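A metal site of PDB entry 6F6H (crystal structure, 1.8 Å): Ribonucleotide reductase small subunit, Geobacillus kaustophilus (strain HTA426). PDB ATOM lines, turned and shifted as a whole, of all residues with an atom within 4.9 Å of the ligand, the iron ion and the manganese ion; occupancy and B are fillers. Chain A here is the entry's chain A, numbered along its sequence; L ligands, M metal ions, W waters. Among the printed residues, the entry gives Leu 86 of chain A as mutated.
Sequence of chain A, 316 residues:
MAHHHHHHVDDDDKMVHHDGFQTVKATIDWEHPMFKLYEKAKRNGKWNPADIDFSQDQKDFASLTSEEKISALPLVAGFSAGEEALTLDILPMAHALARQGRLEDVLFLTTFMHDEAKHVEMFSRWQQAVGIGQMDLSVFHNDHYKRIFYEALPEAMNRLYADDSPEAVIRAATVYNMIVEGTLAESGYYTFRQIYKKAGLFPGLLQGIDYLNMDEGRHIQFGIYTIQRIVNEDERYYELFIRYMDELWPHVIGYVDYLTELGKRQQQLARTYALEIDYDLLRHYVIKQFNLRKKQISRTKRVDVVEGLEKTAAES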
ATOM      1  N   LEU A  75      24.747   6.840 -23.049  1.00  0.00           N
ATOM      2  CA  LEU A  75      24.845   8.254 -22.751  1.00  0.00           C
ATOM      3  C   LEU A  75      23.485   8.932 -22.892  1.00  0.00           C
ATOM      4  O   LEU A  75      23.099   9.721 -22.015  1.00  0.00           O
ATOM      5  CB  LEU A  75      25.879   8.906 -23.677  1.00  0.00           C
ATOM      6  CG  LEU A  75      26.520  10.218 -23.197  1.00  0.00           C
ATOM      7  CD1 LEU A  75      27.306   9.977 -21.889  1.00  0.00           C
ATOM      8  CD2 LEU A  75      27.438  10.804 -24.254  1.00  0.00           C
ATOM      9  N   GLY A  78      21.287   8.101 -20.010  1.00  0.00           N
ATOM     10  CA  GLY A  78      21.635   8.823 -18.804  1.00  0.00           C
ATOM     11  C   GLY A  78      21.073  10.230 -18.825  1.00  0.00           C
ATOM     12  O   GLY A  78      20.526  10.705 -17.825  1.00  0.00           O
ATOM     13  N   PHE A  79      21.193  10.910 -19.973  1.00  0.00           N
ATOM     14  CA  PHE A  79      20.641  12.258 -20.078  1.00  0.00           C
ATOM     15  C   PHE A  79      19.124  12.236 -20.018  1.00  0.00           C
ATOM     16  O   PHE A  79      18.523  13.055 -19.304  1.00  0.00           O
ATOM     17  CB  PHE A  79      21.084  12.937 -21.371  1.00  0.00           C
ATOM     18  CG  PHE A  79      22.324  13.787 -21.198  1.00  0.00           C
ATOM     19  CD1 PHE A  79      22.242  15.060 -20.654  1.00  0.00           C
ATOM     20  CD2 PHE A  79      23.565  13.299 -21.569  1.00  0.00           C
ATOM     21  CE1 PHE A  79      23.407  15.823 -20.484  1.00  0.00           C
ATOM     22  CE2 PHE A  79      24.717  14.060 -21.416  1.00  0.00           C
ATOM     23  CZ  PHE A  79      24.633  15.300 -20.873  1.00  0.00           C
ATOM     24  N   GLY A  82      17.925  11.912 -16.601  1.00  0.00           N
ATOM     25  CA  GLY A  82      18.368  13.118 -15.898  1.00  0.00           C
ATOM     26  C   GLY A  82      17.485  14.326 -16.159  1.00  0.00           C
ATOM     27  O   GLY A  82      17.039  14.999 -15.226  1.00  0.00           O
ATOM     28  N   GLU A  83      17.247  14.641 -17.435  1.00  0.00           N
ATOM     29  CA  GLU A  83      16.372  15.757 -17.780  1.00  0.00           C
ATOM     30  C   GLU A  83      15.001  15.603 -17.146  1.00  0.00           C
ATOM     31  O   GLU A  83      14.421  16.582 -16.620  1.00  0.00           O
ATOM     32  CB  GLU A  83      16.197  15.881 -19.303  1.00  0.00           C
ATOM     33  CG  GLU A  83      17.492  15.953 -20.128  1.00  0.00           C
ATOM     34  CD  GLU A  83      18.466  17.053 -19.705  1.00  0.00           C
ATOM     35  OE1 GLU A  83      18.071  18.000 -18.988  1.00  0.00           O
ATOM     36  OE2 GLU A  83      19.635  16.990 -20.141  1.00  0.00           O
ATOM     37  N   LEU A  86      15.164  16.101 -13.391  1.00  0.00           N
ATOM     38  CA  LEU A  86      15.393  17.492 -13.053  1.00  0.00           C
ATOM     39  C   LEU A  86      14.182  18.359 -13.355  1.00  0.00           C
ATOM     40  O   LEU A  86      13.946  19.343 -12.652  1.00  0.00           O
ATOM     41  CB  LEU A  86      16.639  18.002 -13.768  1.00  0.00           C
ATOM     42  CG  LEU A  86      17.901  17.869 -12.900  1.00  0.00           C
ATOM     43  CD1 LEU A  86      18.232  16.502 -12.477  1.00  0.00           C
ATOM     44  CD2 LEU A  86      19.083  18.423 -13.679  1.00  0.00           C
ATOM     45  N   PHE A 112      14.312  28.265 -15.334  1.00  0.00           N
ATOM     46  CA  PHE A 112      15.013  27.011 -15.041  1.00  0.00           C
ATOM     47  C   PHE A 112      14.121  25.805 -15.390  1.00  0.00           C
ATOM     48  O   PHE A 112      14.539  24.885 -16.115  1.00  0.00           O
ATOM     49  CB  PHE A 112      15.411  27.042 -13.547  1.00  0.00           C
ATOM     50  CG  PHE A 112      16.481  26.068 -13.137  1.00  0.00           C
ATOM     51  CD1 PHE A 112      17.376  26.399 -12.153  1.00  0.00           C
ATOM     52  CD2 PHE A 112      16.524  24.776 -13.639  1.00  0.00           C
ATOM     53  CE1 PHE A 112      18.360  25.515 -11.762  1.00  0.00           C
ATOM     54  CE2 PHE A 112      17.493  23.886 -13.236  1.00  0.00           C
ATOM     55  CZ  PHE A 112      18.430  24.267 -12.310  1.00  0.00           C
ATOM     56  N   GLU A 116      14.515  22.814 -18.442  1.00  0.00           N
ATOM     57  CA  GLU A 116      14.632  21.373 -18.266  1.00  0.00           C
ATOM     58  C   GLU A 116      13.530  20.634 -19.028  1.00  0.00           C
ATOM     59  O   GLU A 116      13.772  19.553 -19.581  1.00  0.00           O
ATOM     60  CB  GLU A 116      14.589  21.016 -16.760  1.00  0.00           C
ATOM     61  CG  GLU A 116      15.728  21.691 -15.962  1.00  0.00           C
ATOM     62  CD  GLU A 116      17.133  21.180 -16.249  1.00  0.00           C
ATOM     63  OE1 GLU A 116      17.349  20.347 -17.165  1.00  0.00           O
ATOM     64  OE2 GLU A 116      18.049  21.658 -15.562  1.00  0.00           O
ATOM     65  N   HIS A 119      14.802  20.374 -22.419  1.00  0.00           N
ATOM     66  CA  HIS A 119      15.806  19.314 -22.462  1.00  0.00           C
ATOM     67  C   HIS A 119      15.179  17.924 -22.584  1.00  0.00           C
ATOM     68  O   HIS A 119      15.644  17.099 -23.392  1.00  0.00           O
ATOM     69  CB  HIS A 119      16.679  19.408 -21.225  1.00  0.00           C
ATOM     70  CG  HIS A 119      17.400  20.708 -21.107  1.00  0.00           C
ATOM     71  ND1 HIS A 119      18.370  20.951 -20.151  1.00  0.00           N
ATOM     72  CD2 HIS A 119      17.334  21.834 -21.862  1.00  0.00           C
ATOM     73  CE1 HIS A 119      18.837  22.186 -20.295  1.00  0.00           C
ATOM     74  NE2 HIS A 119      18.226  22.736 -21.331  1.00  0.00           N
ATOM     75  N   TYR A 145      24.010   4.937 -10.813  1.00  0.00           N
ATOM     76  CA  TYR A 145      23.110   5.909 -11.429  1.00  0.00           C
ATOM     77  C   TYR A 145      21.792   5.994 -10.648  1.00  0.00           C
ATOM     78  O   TYR A 145      21.285   7.083 -10.370  1.00  0.00           O
ATOM     79  CB  TYR A 145      22.870   5.555 -12.886  1.00  0.00           C
ATOM     80  CG  TYR A 145      22.058   6.568 -13.609  1.00  0.00           C
ATOM     81  CD1 TYR A 145      22.665   7.579 -14.342  1.00  0.00           C
ATOM     82  CD2 TYR A 145      20.685   6.509 -13.617  1.00  0.00           C
ATOM     83  CE1 TYR A 145      21.923   8.508 -15.013  1.00  0.00           C
ATOM     84  CE2 TYR A 145      19.928   7.433 -14.276  1.00  0.00           C
ATOM     85  CZ  TYR A 145      20.562   8.427 -14.999  1.00  0.00           C
ATOM     86  OH  TYR A 145      19.832   9.358 -15.651  1.00  0.00           O
ATOM     87  N   PHE A 149      19.931   9.342  -9.243  1.00  0.00           N
ATOM     88  CA  PHE A 149      18.773   9.916  -9.924  1.00  0.00           C
ATOM     89  C   PHE A 149      17.421   9.351  -9.475  1.00  0.00           C
ATOM     90  O   PHE A 149      16.411  10.072  -9.514  1.00  0.00           O
ATOM     91  CB  PHE A 149      18.941   9.710 -11.427  1.00  0.00           C
ATOM     92  CG  PHE A 149      19.981  10.621 -12.019  1.00  0.00           C
ATOM     93  CD1 PHE A 149      19.648  11.902 -12.381  1.00  0.00           C
ATOM     94  CD2 PHE A 149      21.288  10.191 -12.172  1.00  0.00           C
ATOM     95  CE1 PHE A 149      20.603  12.746 -12.927  1.00  0.00           C
ATOM     96  CE2 PHE A 149      22.236  11.041 -12.707  1.00  0.00           C
ATOM     97  CZ  PHE A 149      21.896  12.317 -13.081  1.00  0.00           C
ATOM     98  N   VAL A 180      24.764  16.754 -10.099  1.00  0.00           N
ATOM     99  CA  VAL A 180      24.093  16.320 -11.335  1.00  0.00           C
ATOM    100  C   VAL A 180      24.412  17.271 -12.473  1.00  0.00           C
ATOM    101  O   VAL A 180      24.824  16.841 -13.558  1.00  0.00           O
ATOM    102  CB  VAL A 180      22.593  16.170 -11.107  1.00  0.00           C
ATOM    103  CG1 VAL A 180      21.885  15.891 -12.405  1.00  0.00           C
ATOM    104  CG2 VAL A 180      22.334  15.013 -10.073  1.00  0.00           C
ATOM    105  N   GLU A 181      24.199  18.573 -12.276  1.00  0.00           N
ATOM    106  CA  GLU A 181      24.450  19.544 -13.340  1.00  0.00           C
ATOM    107  C   GLU A 181      25.939  19.847 -13.493  1.00  0.00           C
ATOM    108  O   GLU A 181      26.511  19.736 -14.595  1.00  0.00           O
ATOM    109  CB  GLU A 181      23.669  20.834 -13.051  1.00  0.00           C
ATOM    110  CG  GLU A 181      22.189  20.652 -13.344  1.00  0.00           C
ATOM    111  CD  GLU A 181      21.300  21.821 -13.030  1.00  0.00           C
ATOM    112  OE1 GLU A 181      21.578  22.537 -12.056  1.00  0.00           O
ATOM    113  OE2 GLU A 181      20.281  22.004 -13.764  1.00  0.00           O
ATOM    114  N   LEU A 184      28.109  15.820 -13.613  1.00  0.00           N
ATOM    115  CA  LEU A 184      27.719  14.827 -14.609  1.00  0.00           C
ATOM    116  C   LEU A 184      27.282  15.465 -15.941  1.00  0.00           C
ATOM    117  O   LEU A 184      27.766  15.067 -17.004  1.00  0.00           O
ATOM    118  CB  LEU A 184      26.626  13.929 -14.063  1.00  0.00           C
ATOM    119  CG  LEU A 184      27.085  12.964 -12.994  1.00  0.00           C
ATOM    120  CD1 LEU A 184      25.836  12.252 -12.410  1.00  0.00           C
ATOM    121  CD2 LEU A 184      28.035  11.943 -13.584  1.00  0.00           C
ATOM    122  N   ALA A 185      26.368  16.445 -15.922  1.00  0.00           N
ATOM    123  CA  ALA A 185      25.879  16.960 -17.209  1.00  0.00           C
ATOM    124  C   ALA A 185      27.009  17.592 -17.986  1.00  0.00           C
ATOM    125  O   ALA A 185      27.116  17.402 -19.202  1.00  0.00           O
ATOM    126  CB  ALA A 185      24.787  17.992 -17.038  1.00  0.00           C
ATOM    127  N   SER A 187      30.133  16.924 -17.912  1.00  0.00           N
ATOM    128  CA  SER A 187      31.030  15.922 -18.427  1.00  0.00           C
ATOM    129  C   SER A 187      30.370  15.154 -19.551  1.00  0.00           C
ATOM    130  O   SER A 187      31.049  14.734 -20.487  1.00  0.00           O
ATOM    131  CB  SER A 187      31.501  15.018 -17.279  1.00  0.00           C
ATOM    132  OG  SER A 187      32.179  15.792 -16.301  1.00  0.00           O
ATOM    133  N   GLY A 188      29.034  15.032 -19.523  1.00  0.00           N
ATOM    134  CA  GLY A 188      28.300  14.482 -20.656  1.00  0.00           C
ATOM    135  C   GLY A 188      28.409  15.338 -21.909  1.00  0.00           C
ATOM    136  O   GLY A 188      28.591  14.812 -23.015  1.00  0.00           O
ATOM    137  N   TYR A 189      28.222  16.658 -21.771  1.00  0.00           N
ATOM    138  CA  TYR A 189      28.364  17.552 -22.946  1.00  0.00           C
ATOM    139  C   TYR A 189      29.731  17.386 -23.565  1.00  0.00           C
ATOM    140  O   TYR A 189      29.873  17.300 -24.791  1.00  0.00           O
ATOM    141  CB  TYR A 189      28.167  19.021 -22.546  1.00  0.00           C
ATOM    142  CG  TYR A 189      26.846  19.305 -21.896  1.00  0.00           C
ATOM    143  CD1 TYR A 189      25.704  18.652 -22.311  1.00  0.00           C
ATOM    144  CD2 TYR A 189      26.725  20.228 -20.849  1.00  0.00           C
ATOM    145  CE1 TYR A 189      24.489  18.877 -21.704  1.00  0.00           C
ATOM    146  CE2 TYR A 189      25.532  20.457 -20.229  1.00  0.00           C
ATOM    147  CZ  TYR A 189      24.390  19.783 -20.670  1.00  0.00           C
ATOM    148  OH  TYR A 189      23.168  19.987 -20.066  1.00  0.00           O
ATOM    149  N   THR A 191      31.831  14.813 -23.281  1.00  0.00           N
ATOM    150  CA  THR A 191      31.944  13.494 -23.891  1.00  0.00           C
ATOM    151  C   THR A 191      31.267  13.442 -25.264  1.00  0.00           C
ATOM    152  O   THR A 191      31.827  12.878 -26.219  1.00  0.00           O
ATOM    153  CB  THR A 191      31.341  12.445 -22.947  1.00  0.00           C
ATOM    154  OG1 THR A 191      32.108  12.393 -21.729  1.00  0.00           O
ATOM    155  CG2 THR A 191      31.344  11.063 -23.560  1.00  0.00           C
ATOM    156  N   GLU A 216      22.737  25.305 -19.152  1.00  0.00           N
ATOM    157  CA  GLU A 216      23.372  24.786 -17.932  1.00  0.00           C
ATOM    158  C   GLU A 216      24.173  25.842 -17.190  1.00  0.00           C
ATOM    159  O   GLU A 216      24.253  25.824 -15.965  1.00  0.00           O
ATOM    160  CB  GLU A 216      24.298  23.625 -18.261  1.00  0.00           C
ATOM    161  CG  GLU A 216      24.396  22.575 -17.188  1.00  0.00           C
ATOM    162  CD  GLU A 216      23.057  21.928 -17.001  1.00  0.00           C
ATOM    163  OE1 GLU A 216      22.770  20.959 -17.714  1.00  0.00           O
ATOM    164  OE2 GLU A 216      22.283  22.433 -16.166  1.00  0.00           O
ATOM    165  N   HIS A 219      21.900  27.363 -14.790  1.00  0.00           N
ATOM    166  CA  HIS A 219      21.474  26.439 -13.744  1.00  0.00           C
ATOM    167  C   HIS A 219      22.552  26.299 -12.674  1.00  0.00           C
ATOM    168  O   HIS A 219      22.274  26.353 -11.470  1.00  0.00           O
ATOM    169  CB  HIS A 219      21.111  25.085 -14.377  1.00  0.00           C
ATOM    170  CG  HIS A 219      20.052  25.190 -15.422  1.00  0.00           C
ATOM    171  ND1 HIS A 219      19.558  24.105 -16.117  1.00  0.00           N
ATOM    172  CD2 HIS A 219      19.381  26.268 -15.878  1.00  0.00           C
ATOM    173  CE1 HIS A 219      18.607  24.514 -16.946  1.00  0.00           C
ATOM    174  NE2 HIS A 219      18.499  25.821 -16.832  1.00  0.00           N
ATOM    175  N   TYR A 255      29.286   5.414 -11.735  1.00  0.00           N
ATOM    176  CA  TYR A 255      28.536   5.469 -12.983  1.00  0.00           C
ATOM    177  C   TYR A 255      29.473   5.703 -14.165  1.00  0.00           C
ATOM    178  O   TYR A 255      29.372   5.033 -15.195  1.00  0.00           O
ATOM    179  CB  TYR A 255      27.482   6.548 -12.911  1.00  0.00           C
ATOM    180  CG  TYR A 255      26.732   6.809 -14.215  1.00  0.00           C
ATOM    181  CD1 TYR A 255      26.011   5.824 -14.833  1.00  0.00           C
ATOM    182  CD2 TYR A 255      26.693   8.070 -14.750  1.00  0.00           C
ATOM    183  CE1 TYR A 255      25.298   6.055 -15.966  1.00  0.00           C
ATOM    184  CE2 TYR A 255      25.978   8.321 -15.944  1.00  0.00           C
ATOM    185  CZ  TYR A 255      25.290   7.318 -16.529  1.00  0.00           C
ATOM    186  OH  TYR A 255      24.564   7.556 -17.675  1.00  0.00           O
ATOM    187  N   VAL A 256      30.413   6.632 -14.004  1.00  0.00           N
ATOM    188  CA  VAL A 256      31.341   6.960 -15.084  1.00  0.00           C
ATOM    189  C   VAL A 256      32.167   5.730 -15.474  1.00  0.00           C
ATOM    190  O   VAL A 256      32.368   5.465 -16.655  1.00  0.00           O
ATOM    191  CB  VAL A 256      32.234   8.140 -14.662  1.00  0.00           C
ATOM    192  CG1 VAL A 256      33.442   8.245 -15.550  1.00  0.00           C
ATOM    193  CG2 VAL A 256      31.444   9.446 -14.651  1.00  0.00           C
ATOM    194  N   LEU A 259      29.920   3.466 -17.614  1.00  0.00           N
ATOM    195  CA  LEU A 259      29.897   3.941 -18.996  1.00  0.00           C
ATOM    196  C   LEU A 259      31.226   3.646 -19.691  1.00  0.00           C
ATOM    197  O   LEU A 259      31.245   3.305 -20.871  1.00  0.00           O
ATOM    198  CB  LEU A 259      29.632   5.436 -19.049  1.00  0.00           C
ATOM    199  CG  LEU A 259      28.226   5.881 -18.675  1.00  0.00           C
ATOM    200  CD1 LEU A 259      28.218   7.405 -18.618  1.00  0.00           C
ATOM    201  CD2 LEU A 259      27.206   5.352 -19.659  1.00  0.00           C
ATOM    202  N   THR A 260      32.337   3.817 -18.979  1.00  0.00           N
ATOM    203  CA  THR A 260      33.644   3.608 -19.577  1.00  0.00           C
ATOM    204  C   THR A 260      33.836   2.158 -19.993  1.00  0.00           C
ATOM    205  O   THR A 260      34.285   1.854 -21.107  1.00  0.00           O
ATOM    206  CB  THR A 260      34.713   4.029 -18.579  1.00  0.00           C
ATOM    207  OG1 THR A 260      34.712   5.453 -18.476  1.00  0.00           O
ATOM    208  CG2 THR A 260      36.075   3.579 -19.031  1.00  0.00           C
ATOM    209  N   TYR A 279      39.359   7.409 -23.002  1.00  0.00           N
ATOM    210  CA  TYR A 279      38.480   7.306 -21.837  1.00  0.00           C
ATOM    211  C   TYR A 279      39.176   7.743 -20.565  1.00  0.00           C
ATOM    212  O   TYR A 279      38.523   8.237 -19.645  1.00  0.00           O
ATOM    213  CB  TYR A 279      37.960   5.895 -21.674  1.00  0.00           C
ATOM    214  CG  TYR A 279      36.982   5.518 -22.720  1.00  0.00           C
ATOM    215  CD1 TYR A 279      35.698   6.059 -22.724  1.00  0.00           C
ATOM    216  CD2 TYR A 279      37.329   4.620 -23.735  1.00  0.00           C
ATOM    217  CE1 TYR A 279      34.795   5.726 -23.702  1.00  0.00           C
ATOM    218  CE2 TYR A 279      36.432   4.283 -24.707  1.00  0.00           C
ATOM    219  CZ  TYR A 279      35.177   4.831 -24.703  1.00  0.00           C
ATOM    220  OH  TYR A 279      34.295   4.482 -25.696  1.00  0.00           O
ATOM    221  N   LEU A 282      38.501  11.345 -20.436  1.00  0.00           N
ATOM    222  CA  LEU A 282      37.156  11.677 -20.018  1.00  0.00           C
ATOM    223  C   LEU A 282      36.997  11.517 -18.520  1.00  0.00           C
ATOM    224  O   LEU A 282      36.417  12.384 -17.860  1.00  0.00           O
ATOM    225  CB  LEU A 282      36.139  10.807 -20.766  1.00  0.00           C
ATOM    226  CG  LEU A 282      36.126  11.055 -22.275  1.00  0.00           C
ATOM    227  CD1 LEU A 282      35.237  10.103 -22.997  1.00  0.00           C
ATOM    228  CD2 LEU A 282      35.730  12.491 -22.631  1.00  0.00           C
ATOM    229  N   VAL A 286      35.934  14.491 -15.563  1.00  0.00           N
ATOM    230  CA  VAL A 286      34.900  14.374 -14.523  1.00  0.00           C
ATOM    231  C   VAL A 286      35.465  14.722 -13.157  1.00  0.00           C
ATOM    232  O   VAL A 286      34.891  15.542 -12.424  1.00  0.00           O
ATOM    233  CB  VAL A 286      34.300  12.961 -14.534  1.00  0.00           C
ATOM    234  CG1 VAL A 286      33.336  12.765 -13.336  1.00  0.00           C
ATOM    235  CG2 VAL A 286      33.573  12.720 -15.839  1.00  0.00           C
HETATM  236  C1  LIG L   1      20.449  18.646 -16.496  1.00  0.00           C
HETATM  237  O1  LIG L   1      19.457  18.409 -17.238  1.00  0.00           O
HETATM  238  O2  LIG L   1      20.851  19.762 -15.993  1.00  0.00           O
HETATM  239  C2  LIG L   1      21.262  17.413 -16.049  1.00  0.00           C
HETATM  240  C3  LIG L   1      21.037  16.116 -16.800  1.00  0.00           C
HETATM  241  C4  LIG L   1      21.774  14.924 -16.141  1.00  0.00           C
HETATM  242  C5  LIG L   1      22.697  14.163 -17.072  1.00  0.00           C
HETATM  243  C6  LIG L   1      23.265  12.877 -16.508  1.00  0.00           C
HETATM  244  C7  LIG L   1      23.913  11.985 -17.570  1.00  0.00           C
HETATM  245  C8  LIG L   1      25.260  12.459 -18.016  1.00  0.00           C
HETATM  246  C9  LIG L   1      26.262  11.364 -18.369  1.00  0.00           C
HETATM  247  C10 LIG L   1      27.626  11.574 -17.701  1.00  0.00           C
HETATM  248  C11 LIG L   1      28.760  11.118 -18.558  1.00  0.00           C
HETATM  249  C12 LIG L   1      30.111  11.326 -17.908  1.00  0.00           C
HETATM  250  C13 LIG L   1      31.290  10.895 -18.794  1.00  0.00           C
HETATM  251  C14 LIG L   1      31.489   9.396 -18.932  1.00  0.00           C
HETATM  252  C15 LIG L   1      32.609   8.981 -19.872  1.00  0.00           C
HETATM  253  C16 LIG L   1      32.285   7.770 -20.748  1.00  0.00           C
HETATM  254 FE    FE M   1      20.089  21.903 -15.843  1.00  0.00          FE
HETATM  255 MN    MN M   2      18.998  19.722 -18.333  1.00  0.00          MN
HETATM  256  O   HOH W   1      20.265  21.377 -17.916  1.00  0.00           O
HETATM  257  O   HOH W   2      20.712  18.845 -19.604  1.00  0.00           O
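OE2 of Glu 116 binds the iron ion (2.1 Å). OE2 of Glu 181 binds the iron ion, 2.1 Å away. Water W1 is bound to the iron ion (2.1 Å). The iron ion is bound by O2 of the ligand, 2.3 Å away. OE2 of Glu 216 is bound to the iron ion (2.3 Å). A ring nitrogen (ND1) of His 219 is bound to the iron ion (2.3 Å).
Within 4 Å of the manganese ion: Glu 83, Glu 116 and His 119. The nearest printed residue that does not touch the manganese ion is Glu 216 (4.02 Å).
The manganese ion is bound by an oxygen (O1) of the ligand (1.8 Å), the side-chain carboxylate of Glu 83 (2.1 Å), the side-chain carboxylate of Glu 116 (2.1 Å), water W1 (2.1 Å), a ring nitrogen (ND1) of His 119 (2.3 Å) and water W2 (2.3 Å).
Merely in contact with the ligand: Leu 86, Thr 191, Leu 184, Gly 78, Ala 185, Phe 79, Phe 149, Leu 259, Leu 75, Val 180, Gly 82, Tyr 255, Val 256, Gly 188 and Ser 187. Hydrophobic or aromatic side chains within 4 Å of the ligand: Leu 75, Phe 79, Leu 86, Phe 149, Val 180, Ala 185, Tyr 255, Val 256 and Leu 259. The nearest printed residue that does not touch the ligand is His 119 (4.02 Å).
Within 4 Å of the iron ion: Glu 116, Glu 181, Glu 216 and His 219. The nearest printed residue that does not touch the iron ion is Phe 112 (4.2 Å).
The side-chain carboxylate (OE1) of Glu 216 lies within hydrogen-bond range of the side-chain hydroxyl (OH) of Tyr 189 (2.6 Å). The side-chain hydroxyl of Thr 191 sits at hydrogen-bond distance from the backbone carbonyl oxygen of Ser 187, at 2.9 Å. O of Gly 78 is in hydrogen-bond range of OH of Tyr 145, at 2.6 Å. O of Val 180 is in hydrogen-bond range of N of Ala 185 (2.9 Å). The side-chain hydroxyl of Tyr 145 sits at hydrogen-bond distance from the backbone NH of Gly 82, at 3.3 Å. O of Val 256 is in hydrogen-bond range of OG1 of Thr 260, at 3.0 Å.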
